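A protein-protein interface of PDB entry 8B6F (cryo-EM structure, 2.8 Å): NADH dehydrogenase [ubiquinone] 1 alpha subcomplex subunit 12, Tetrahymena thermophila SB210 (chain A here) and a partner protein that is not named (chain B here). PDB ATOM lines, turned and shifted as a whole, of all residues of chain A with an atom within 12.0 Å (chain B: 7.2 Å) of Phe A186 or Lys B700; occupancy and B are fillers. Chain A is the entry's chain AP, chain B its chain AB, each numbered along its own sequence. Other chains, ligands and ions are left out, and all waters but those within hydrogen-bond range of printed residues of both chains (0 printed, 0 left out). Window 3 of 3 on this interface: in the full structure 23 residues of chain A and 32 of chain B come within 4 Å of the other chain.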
ATOM      1  N   ALA A 181      11.512 -19.957 -10.645  1.00  0.00           N
ATOM      2  CA  ALA A 181      10.963 -19.982 -11.991  1.00  0.00           C
ATOM      3  C   ALA A 181       9.771 -19.041 -12.099  1.00  0.00           C
ATOM      4  O   ALA A 181       9.010 -18.851 -11.146  1.00  0.00           O
ATOM      5  CB  ALA A 181      10.543 -21.403 -12.370  1.00  0.00           C
ATOM      6  N   SER A 182       9.615 -18.442 -13.276  1.00  0.00           N
ATOM      7  CA  SER A 182       8.510 -17.522 -13.503  1.00  0.00           C
ATOM      8  C   SER A 182       7.182 -18.266 -13.461  1.00  0.00           C
ATOM      9  O   SER A 182       7.049 -19.366 -14.006  1.00  0.00           O
ATOM     10  CB  SER A 182       8.673 -16.814 -14.848  1.00  0.00           C
ATOM     11  OG  SER A 182       8.624 -17.740 -15.920  1.00  0.00           O
ATOM     12  N   ASN A 183       6.197 -17.660 -12.807  1.00  0.00           N
ATOM     13  CA  ASN A 183       4.870 -18.245 -12.672  1.00  0.00           C
ATOM     14  C   ASN A 183       3.895 -17.758 -13.737  1.00  0.00           C
ATOM     15  O   ASN A 183       2.712 -18.108 -13.677  1.00  0.00           O
ATOM     16  CB  ASN A 183       4.299 -17.940 -11.284  1.00  0.00           C
ATOM     17  CG  ASN A 183       4.069 -16.458 -11.063  1.00  0.00           C
ATOM     18  OD1 ASN A 183       4.945 -15.748 -10.572  1.00  0.00           O
ATOM     19  ND2 ASN A 183       2.882 -15.983 -11.425  1.00  0.00           N
ATOM     20  N   SER A 184       4.353 -16.966 -14.696  1.00  0.00           N
ATOM     21  CA  SER A 184       3.459 -16.424 -15.712  1.00  0.00           C
ATOM     22  C   SER A 184       2.946 -17.542 -16.610  1.00  0.00           C
ATOM     23  O   SER A 184       3.756 -18.240 -17.234  1.00  0.00           O
ATOM     24  CB  SER A 184       4.188 -15.377 -16.547  1.00  0.00           C
ATOM     25  OG  SER A 184       4.674 -14.324 -15.732  1.00  0.00           O
ATOM     26  N   PRO A 185       1.631 -17.755 -16.709  1.00  0.00           N
ATOM     27  CA  PRO A 185       1.134 -18.795 -17.622  1.00  0.00           C
ATOM     28  C   PRO A 185       1.513 -18.554 -19.070  1.00  0.00           C
ATOM     29  O   PRO A 185       1.694 -19.519 -19.824  1.00  0.00           O
ATOM     30  CB  PRO A 185      -0.387 -18.741 -17.423  1.00  0.00           C
ATOM     31  CG  PRO A 185      -0.580 -18.124 -16.088  1.00  0.00           C
ATOM     32  CD  PRO A 185       0.540 -17.149 -15.924  1.00  0.00           C
ATOM     33  N   PHE A 186       1.638 -17.296 -19.483  1.00  0.00           N
ATOM     34  CA  PHE A 186       1.914 -16.992 -20.879  1.00  0.00           C
ATOM     35  C   PHE A 186       3.285 -17.517 -21.285  1.00  0.00           C
ATOM     36  O   PHE A 186       4.227 -17.551 -20.490  1.00  0.00           O
ATOM     37  CB  PHE A 186       1.836 -15.485 -21.118  1.00  0.00           C
ATOM     38  CG  PHE A 186       0.496 -14.894 -20.803  1.00  0.00           C
ATOM     39  CD1 PHE A 186      -0.516 -14.903 -21.748  1.00  0.00           C
ATOM     40  CD2 PHE A 186       0.246 -14.333 -19.562  1.00  0.00           C
ATOM     41  CE1 PHE A 186      -1.753 -14.363 -21.461  1.00  0.00           C
ATOM     42  CE2 PHE A 186      -0.989 -13.790 -19.269  1.00  0.00           C
ATOM     43  CZ  PHE A 186      -1.989 -13.805 -20.221  1.00  0.00           C
ATOM     44  N   ILE A 187       3.386 -17.924 -22.540  1.00  0.00           N
ATOM     45  CA  ILE A 187       4.606 -18.506 -23.083  1.00  0.00           C
ATOM     46  C   ILE A 187       5.458 -17.402 -23.689  1.00  0.00           C
ATOM     47  O   ILE A 187       4.953 -16.515 -24.386  1.00  0.00           O
ATOM     48  CB  ILE A 187       4.269 -19.589 -24.125  1.00  0.00           C
ATOM     49  CG1 ILE A 187       3.481 -20.726 -23.468  1.00  0.00           C
ATOM     50  CG2 ILE A 187       5.536 -20.127 -24.765  1.00  0.00           C
ATOM     51  CD1 ILE A 187       2.937 -21.749 -24.445  1.00  0.00           C
ATOM     52  N   ASP A 188       6.763 -17.456 -23.420  1.00  0.00           N
ATOM     53  CA  ASP A 188       7.720 -16.506 -23.985  1.00  0.00           C
ATOM     54  C   ASP A 188       8.126 -17.015 -25.366  1.00  0.00           C
ATOM     55  O   ASP A 188       9.158 -17.660 -25.557  1.00  0.00           O
ATOM     56  CB  ASP A 188       8.922 -16.339 -23.065  1.00  0.00           C
ATOM     57  CG  ASP A 188       9.818 -15.189 -23.481  1.00  0.00           C
ATOM     58  OD1 ASP A 188       9.493 -14.511 -24.478  1.00  0.00           O
ATOM     59  OD2 ASP A 188      10.848 -14.964 -22.812  1.00  0.00           O
ATOM     60  N   ASP A 189       7.279 -16.710 -26.350  1.00  0.00           N
ATOM     61  CA  ASP A 189       7.482 -17.236 -27.697  1.00  0.00           C
ATOM     62  C   ASP A 189       8.790 -16.738 -28.300  1.00  0.00           C
ATOM     63  O   ASP A 189       9.498 -17.496 -28.972  1.00  0.00           O
ATOM     64  CB  ASP A 189       6.301 -16.856 -28.590  1.00  0.00           C
ATOM     65  CG  ASP A 189       6.099 -15.357 -28.684  1.00  0.00           C
ATOM     66  OD1 ASP A 189       6.437 -14.648 -27.712  1.00  0.00           O
ATOM     67  OD2 ASP A 189       5.601 -14.886 -29.727  1.00  0.00           O
ATOM     68  N   MET A 190       9.129 -15.469 -28.070  1.00  0.00           N
ATOM     69  CA  MET A 190      10.355 -14.925 -28.647  1.00  0.00           C
ATOM     70  C   MET A 190      11.584 -15.647 -28.112  1.00  0.00           C
ATOM     71  O   MET A 190      12.508 -15.960 -28.870  1.00  0.00           O
ATOM     72  CB  MET A 190      10.450 -13.426 -28.360  1.00  0.00           C
ATOM     73  CG  MET A 190       9.234 -12.631 -28.815  1.00  0.00           C
ATOM     74  SD  MET A 190       8.748 -12.973 -30.519  1.00  0.00           S
ATOM     75  CE  MET A 190      10.240 -12.537 -31.403  1.00  0.00           C
ATOM     76  N   SER A 191      11.621 -15.916 -26.806  1.00  0.00           N
ATOM     77  CA  SER A 191      12.752 -16.648 -26.248  1.00  0.00           C
ATOM     78  C   SER A 191      12.783 -18.086 -26.754  1.00  0.00           C
ATOM     79  O   SER A 191      13.850 -18.600 -27.108  1.00  0.00           O
ATOM     80  CB  SER A 191      12.693 -16.617 -24.721  1.00  0.00           C
ATOM     81  OG  SER A 191      11.614 -17.399 -24.237  1.00  0.00           O
ATOM     82  N   ILE A 192      11.625 -18.750 -26.800  1.00  0.00           N
ATOM     83  CA  ILE A 192      11.593 -20.154 -27.203  1.00  0.00           C
ATOM     84  C   ILE A 192      12.029 -20.303 -28.655  1.00  0.00           C
ATOM     85  O   ILE A 192      12.798 -21.209 -28.997  1.00  0.00           O
ATOM     86  CB  ILE A 192      10.191 -20.747 -26.968  1.00  0.00           C
ATOM     87  CG1 ILE A 192       9.930 -20.879 -25.464  1.00  0.00           C
ATOM     88  CG2 ILE A 192      10.048 -22.101 -27.669  1.00  0.00           C
ATOM     89  CD1 ILE A 192       8.553 -21.398 -25.120  1.00  0.00           C
ATOM     90  N   ARG A 193      11.543 -19.427 -29.529  1.00  0.00           N
ATOM     91  CA  ARG A 193      11.862 -19.508 -30.950  1.00  0.00           C
ATOM     92  C   ARG A 193      12.133 -18.123 -31.521  1.00  0.00           C
ATOM     93  O   ARG A 193      11.233 -17.481 -32.064  1.00  0.00           O
ATOM     94  CB  ARG A 193      10.718 -20.180 -31.713  1.00  0.00           C
ATOM     95  CG  ARG A 193      10.943 -20.315 -33.217  1.00  0.00           C
ATOM     96  CD  ARG A 193      12.092 -21.261 -33.542  1.00  0.00           C
ATOM     97  NE  ARG A 193      13.397 -20.628 -33.392  1.00  0.00           N
ATOM     98  CZ  ARG A 193      14.553 -21.231 -33.633  1.00  0.00           C
ATOM     99  NH1 ARG A 193      14.607 -22.491 -34.032  1.00  0.00           N
ATOM    100  NH2 ARG A 193      15.685 -20.551 -33.473  1.00  0.00           N
ATOM    101  N   PRO B 168      -5.443  -8.013 -29.416  1.00  0.00           N
ATOM    102  CA  PRO B 168      -6.004  -8.015 -28.059  1.00  0.00           C
ATOM    103  C   PRO B 168      -6.293  -6.636 -27.491  1.00  0.00           C
ATOM    104  O   PRO B 168      -6.729  -6.545 -26.338  1.00  0.00           O
ATOM    105  CB  PRO B 168      -4.905  -8.716 -27.244  1.00  0.00           C
ATOM    106  CG  PRO B 168      -3.652  -8.381 -27.961  1.00  0.00           C
ATOM    107  CD  PRO B 168      -4.008  -8.342 -29.421  1.00  0.00           C
ATOM    108  N   PRO B 236      -9.488  -5.087 -23.450  1.00  0.00           N
ATOM    109  CA  PRO B 236      -9.248  -5.375 -22.026  1.00  0.00           C
ATOM    110  C   PRO B 236     -10.313  -4.807 -21.108  1.00  0.00           C
ATOM    111  O   PRO B 236     -10.644  -5.431 -20.092  1.00  0.00           O
ATOM    112  CB  PRO B 236      -7.882  -4.729 -21.765  1.00  0.00           C
ATOM    113  CG  PRO B 236      -7.210  -4.736 -23.075  1.00  0.00           C
ATOM    114  CD  PRO B 236      -8.281  -4.558 -24.110  1.00  0.00           C
ATOM    115  N   ARG B 300      -1.837  -6.941  -9.322  1.00  0.00           N
ATOM    116  CA  ARG B 300      -1.323  -8.224  -8.868  1.00  0.00           C
ATOM    117  C   ARG B 300       0.173  -8.119  -8.613  1.00  0.00           C
ATOM    118  O   ARG B 300       0.831  -7.156  -9.015  1.00  0.00           O
ATOM    119  CB  ARG B 300      -1.626  -9.339  -9.875  1.00  0.00           C
ATOM    120  CG  ARG B 300      -0.944  -9.184 -11.223  1.00  0.00           C
ATOM    121  CD  ARG B 300      -0.997 -10.493 -11.987  1.00  0.00           C
ATOM    122  NE  ARG B 300      -0.237 -10.431 -13.228  1.00  0.00           N
ATOM    123  CZ  ARG B 300       0.027 -11.478 -13.996  1.00  0.00           C
ATOM    124  NH1 ARG B 300      -0.387 -12.693 -13.676  1.00  0.00           N
ATOM    125  NH2 ARG B 300       0.723 -11.302 -15.116  1.00  0.00           N
ATOM    126  N   TYR B 686       6.262  -3.703 -24.715  1.00  0.00           N
ATOM    127  CA  TYR B 686       5.206  -3.960 -23.748  1.00  0.00           C
ATOM    128  C   TYR B 686       5.730  -4.430 -22.396  1.00  0.00           C
ATOM    129  O   TYR B 686       4.935  -4.566 -21.461  1.00  0.00           O
ATOM    130  CB  TYR B 686       4.237  -4.998 -24.319  1.00  0.00           C
ATOM    131  CG  TYR B 686       3.682  -4.607 -25.670  1.00  0.00           C
ATOM    132  CD1 TYR B 686       2.742  -3.593 -25.787  1.00  0.00           C
ATOM    133  CD2 TYR B 686       4.104  -5.248 -26.827  1.00  0.00           C
ATOM    134  CE1 TYR B 686       2.235  -3.228 -27.018  1.00  0.00           C
ATOM    135  CE2 TYR B 686       3.603  -4.890 -28.063  1.00  0.00           C
ATOM    136  CZ  TYR B 686       2.669  -3.880 -28.152  1.00  0.00           C
ATOM    137  OH  TYR B 686       2.166  -3.519 -29.378  1.00  0.00           O
ATOM    138  N   MET B 687       7.033  -4.677 -22.266  1.00  0.00           N
ATOM    139  CA  MET B 687       7.635  -5.107 -21.003  1.00  0.00           C
ATOM    140  C   MET B 687       8.907  -4.295 -20.784  1.00  0.00           C
ATOM    141  O   MET B 687       9.960  -4.618 -21.343  1.00  0.00           O
ATOM    142  CB  MET B 687       7.937  -6.602 -21.022  1.00  0.00           C
ATOM    143  CG  MET B 687       6.725  -7.485 -21.263  1.00  0.00           C
ATOM    144  SD  MET B 687       5.455  -7.279 -20.008  1.00  0.00           S
ATOM    145  CE  MET B 687       4.338  -8.604 -20.445  1.00  0.00           C
ATOM    146  N   SER B 695       1.787  -6.979 -15.501  1.00  0.00           N
ATOM    147  CA  SER B 695       0.496  -6.804 -16.152  1.00  0.00           C
ATOM    148  C   SER B 695       0.155  -8.003 -17.030  1.00  0.00           C
ATOM    149  O   SER B 695       1.032  -8.670 -17.584  1.00  0.00           O
ATOM    150  CB  SER B 695       0.489  -5.527 -16.988  1.00  0.00           C
ATOM    151  OG  SER B 695      -0.746  -5.381 -17.665  1.00  0.00           O
ATOM    152  N   VAL B 696      -1.145  -8.269 -17.153  1.00  0.00           N
ATOM    153  CA  VAL B 696      -1.635  -9.364 -17.985  1.00  0.00           C
ATOM    154  C   VAL B 696      -1.925  -8.894 -19.403  1.00  0.00           C
ATOM    155  O   VAL B 696      -1.593  -9.582 -20.371  1.00  0.00           O
ATOM    156  CB  VAL B 696      -2.886  -9.996 -17.340  1.00  0.00           C
ATOM    157  CG1 VAL B 696      -3.440 -11.109 -18.220  1.00  0.00           C
ATOM    158  CG2 VAL B 696      -2.563 -10.522 -15.954  1.00  0.00           C
ATOM    159  N   THR B 697      -2.552  -7.726 -19.549  1.00  0.00           N
ATOM    160  CA  THR B 697      -2.802  -7.185 -20.881  1.00  0.00           C
ATOM    161  C   THR B 697      -1.498  -6.982 -21.641  1.00  0.00           C
ATOM    162  O   THR B 697      -1.429  -7.232 -22.849  1.00  0.00           O
ATOM    163  CB  THR B 697      -3.568  -5.866 -20.776  1.00  0.00           C
ATOM    164  OG1 THR B 697      -4.815  -6.084 -20.104  1.00  0.00           O
ATOM    165  CG2 THR B 697      -3.840  -5.289 -22.160  1.00  0.00           C
ATOM    166  N   MET B 698      -0.449  -6.533 -20.948  1.00  0.00           N
ATOM    167  CA  MET B 698       0.844  -6.363 -21.599  1.00  0.00           C
ATOM    168  C   MET B 698       1.404  -7.703 -22.054  1.00  0.00           C
ATOM    169  O   MET B 698       2.039  -7.792 -23.112  1.00  0.00           O
ATOM    170  CB  MET B 698       1.820  -5.664 -20.653  1.00  0.00           C
ATOM    171  CG  MET B 698       1.304  -4.340 -20.111  1.00  0.00           C
ATOM    172  SD  MET B 698       0.835  -3.161 -21.390  1.00  0.00           S
ATOM    173  CE  MET B 698       2.438  -2.720 -22.042  1.00  0.00           C
ATOM    174  N   ALA B 699       1.188  -8.759 -21.267  1.00  0.00           N
ATOM    175  CA  ALA B 699       1.623 -10.086 -21.688  1.00  0.00           C
ATOM    176  C   ALA B 699       0.872 -10.535 -22.934  1.00  0.00           C
ATOM    177  O   ALA B 699       1.470 -11.098 -23.858  1.00  0.00           O
ATOM    178  CB  ALA B 699       1.425 -11.089 -20.553  1.00  0.00           C
ATOM    179  N   LYS B 700      -0.441 -10.300 -22.980  1.00  0.00           N
ATOM    180  CA  LYS B 700      -1.205 -10.641 -24.175  1.00  0.00           C
ATOM    181  C   LYS B 700      -0.699  -9.862 -25.380  1.00  0.00           C
ATOM    182  O   LYS B 700      -0.547 -10.418 -26.473  1.00  0.00           O
ATOM    183  CB  LYS B 700      -2.693 -10.376 -23.952  1.00  0.00           C
ATOM    184  CG  LYS B 700      -3.363 -11.358 -23.009  1.00  0.00           C
ATOM    185  CD  LYS B 700      -4.856 -11.089 -22.918  1.00  0.00           C
ATOM    186  CE  LYS B 700      -5.524 -12.014 -21.918  1.00  0.00           C
ATOM    187  NZ  LYS B 700      -6.984 -11.741 -21.806  1.00  0.00           N
ATOM    188  N   CYS B 701      -0.442  -8.566 -25.201  1.00  0.00           N
ATOM    189  CA  CYS B 701       0.076  -7.757 -26.298  1.00  0.00           C
ATOM    190  C   CYS B 701       1.435  -8.264 -26.759  1.00  0.00           C
ATOM    191  O   CYS B 701       1.711  -8.318 -27.963  1.00  0.00           O
ATOM    192  CB  CYS B 701       0.179  -6.295 -25.869  1.00  0.00           C
ATOM    193  SG  CYS B 701      -1.402  -5.472 -25.655  1.00  0.00           S
ATOM    194  N   SER B 702       2.302  -8.636 -25.816  1.00  0.00           N
ATOM    195  CA  SER B 702       3.607  -9.169 -26.190  1.00  0.00           C
ATOM    196  C   SER B 702       3.462 -10.426 -27.038  1.00  0.00           C
ATOM    197  O   SER B 702       4.029 -10.519 -28.132  1.00  0.00           O
ATOM    198  CB  SER B 702       4.423  -9.466 -24.931  1.00  0.00           C
ATOM    199  OG  SER B 702       4.622  -8.295 -24.161  1.00  0.00           O
ATOM    200  N   THR B 703       2.707 -11.408 -26.546  1.00  0.00           N
ATOM    201  CA  THR B 703       2.573 -12.659 -27.279  1.00  0.00           C
ATOM    202  C   THR B 703       1.863 -12.473 -28.613  1.00  0.00           C
ATOM    203  O   THR B 703       2.064 -13.281 -29.526  1.00  0.00           O
ATOM    204  CB  THR B 703       1.823 -13.695 -26.437  1.00  0.00           C
ATOM    205  OG1 THR B 703       1.737 -14.933 -27.155  1.00  0.00           O
ATOM    206  CG2 THR B 703       0.422 -13.215 -26.103  1.00  0.00           C
ATOM    207  N   ALA B 704       1.039 -11.433 -28.749  1.00  0.00           N
ATOM    208  CA  ALA B 704       0.305 -11.210 -29.984  1.00  0.00           C
ATOM    209  C   ALA B 704       1.028 -10.317 -30.980  1.00  0.00           C
ATOM    210  O   ALA B 704       0.641 -10.293 -32.153  1.00  0.00           O
ATOM    211  CB  ALA B 704      -1.060 -10.588 -29.672  1.00  0.00           C
ATOM    212  N   PHE B 705       2.059  -9.582 -30.555  1.00  0.00           N
ATOM    213  CA  PHE B 705       2.687  -8.591 -31.415  1.00  0.00           C
ATOM    214  C   PHE B 705       4.185  -8.761 -31.610  1.00  0.00           C
ATOM    215  O   PHE B 705       4.709  -8.270 -32.615  1.00  0.00           O
ATOM    216  CB  PHE B 705       2.440  -7.175 -30.866  1.00  0.00           C
ATOM    217  CG  PHE B 705       0.994  -6.764 -30.859  1.00  0.00           C
ATOM    218  CD1 PHE B 705       0.131  -7.171 -31.863  1.00  0.00           C
ATOM    219  CD2 PHE B 705       0.500  -5.958 -29.846  1.00  0.00           C
ATOM    220  CE1 PHE B 705      -1.195  -6.788 -31.854  1.00  0.00           C
ATOM    221  CE2 PHE B 705      -0.824  -5.571 -29.833  1.00  0.00           C
ATOM    222  CZ  PHE B 705      -1.671  -5.985 -30.840  1.00  0.00           C
ATOM    223  N   ASN B 706       4.891  -9.431 -30.697  1.00  0.00           N
ATOM    224  CA  ASN B 706       6.348  -9.474 -30.801  1.00  0.00           C
ATOM    225  C   ASN B 706       6.792 -10.190 -32.070  1.00  0.00           C
ATOM    226  O   ASN B 706       7.688  -9.720 -32.779  1.00  0.00           O
ATOM    227  CB  ASN B 706       6.943 -10.149 -29.565  1.00  0.00           C
ATOM    228  CG  ASN B 706       6.823  -9.292 -28.322  1.00  0.00           C
ATOM    229  OD1 ASN B 706       6.596  -8.086 -28.405  1.00  0.00           O
ATOM    230  ND2 ASN B 706       6.987  -9.912 -27.160  1.00  0.00           N
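The backbone carbonyl oxygen (O) of Ser B702 lies close to the side-chain amide nitrogen (ND2) of Asn B706 (3.2 Å).
Among the printed residues, pairs that only touch across the chains: Met A190 with Asn B706 (3.5 Å), Phe A186 with Ala B699 (3.6 Å), Phe A186 with Val B696 (3.7 Å), Phe A186 with Lys B700 (3.7 Å) and Asp A189 with Thr B703 (3.9 Å).
Phe A186 touches three residues of chain B. Of the printed residues of chain B, Asp A189 touches Thr B703 (3.9 Å). No residue of chain A comes within 4 Å of Pro B168. No residue of chain A comes within 4 Å of Pro B236. Val B696 touches just one residue of chain A: Phe A186. Of chain A, only Phe A186 (3.6 Å) comes within 4 Å of Ala B699. Lys B700 touches just one residue of chain A: Phe A186 (3.7 Å). No residue of chain A comes within 4 Å of Cys B701. No residue of chain A comes within 4 Å of Ala B704. Of the printed residues of chain A, Asn B706 touches Met A190 (3.5 Å). The nearest residue of chain A that does not touch Lys B700 is Asp A189 (8.3 Å). The nearest printed residue of chain B that does not touch Met A190 is Ser B702 (5.7 Å).
Hydrophobic or aromatic side chains of chain A within 4 Å of the printed part of chain B: Phe A186 and Met A190. Of the 17 printed residues of chain B, 5 touch a printed residue of chain A. Among the printed residues, 5 pairs touch across the chains. Among the printed residues, no Asp or Glu carboxylate lies within 4 Å of a Lys or Arg side-chain nitrogen of the other chain.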
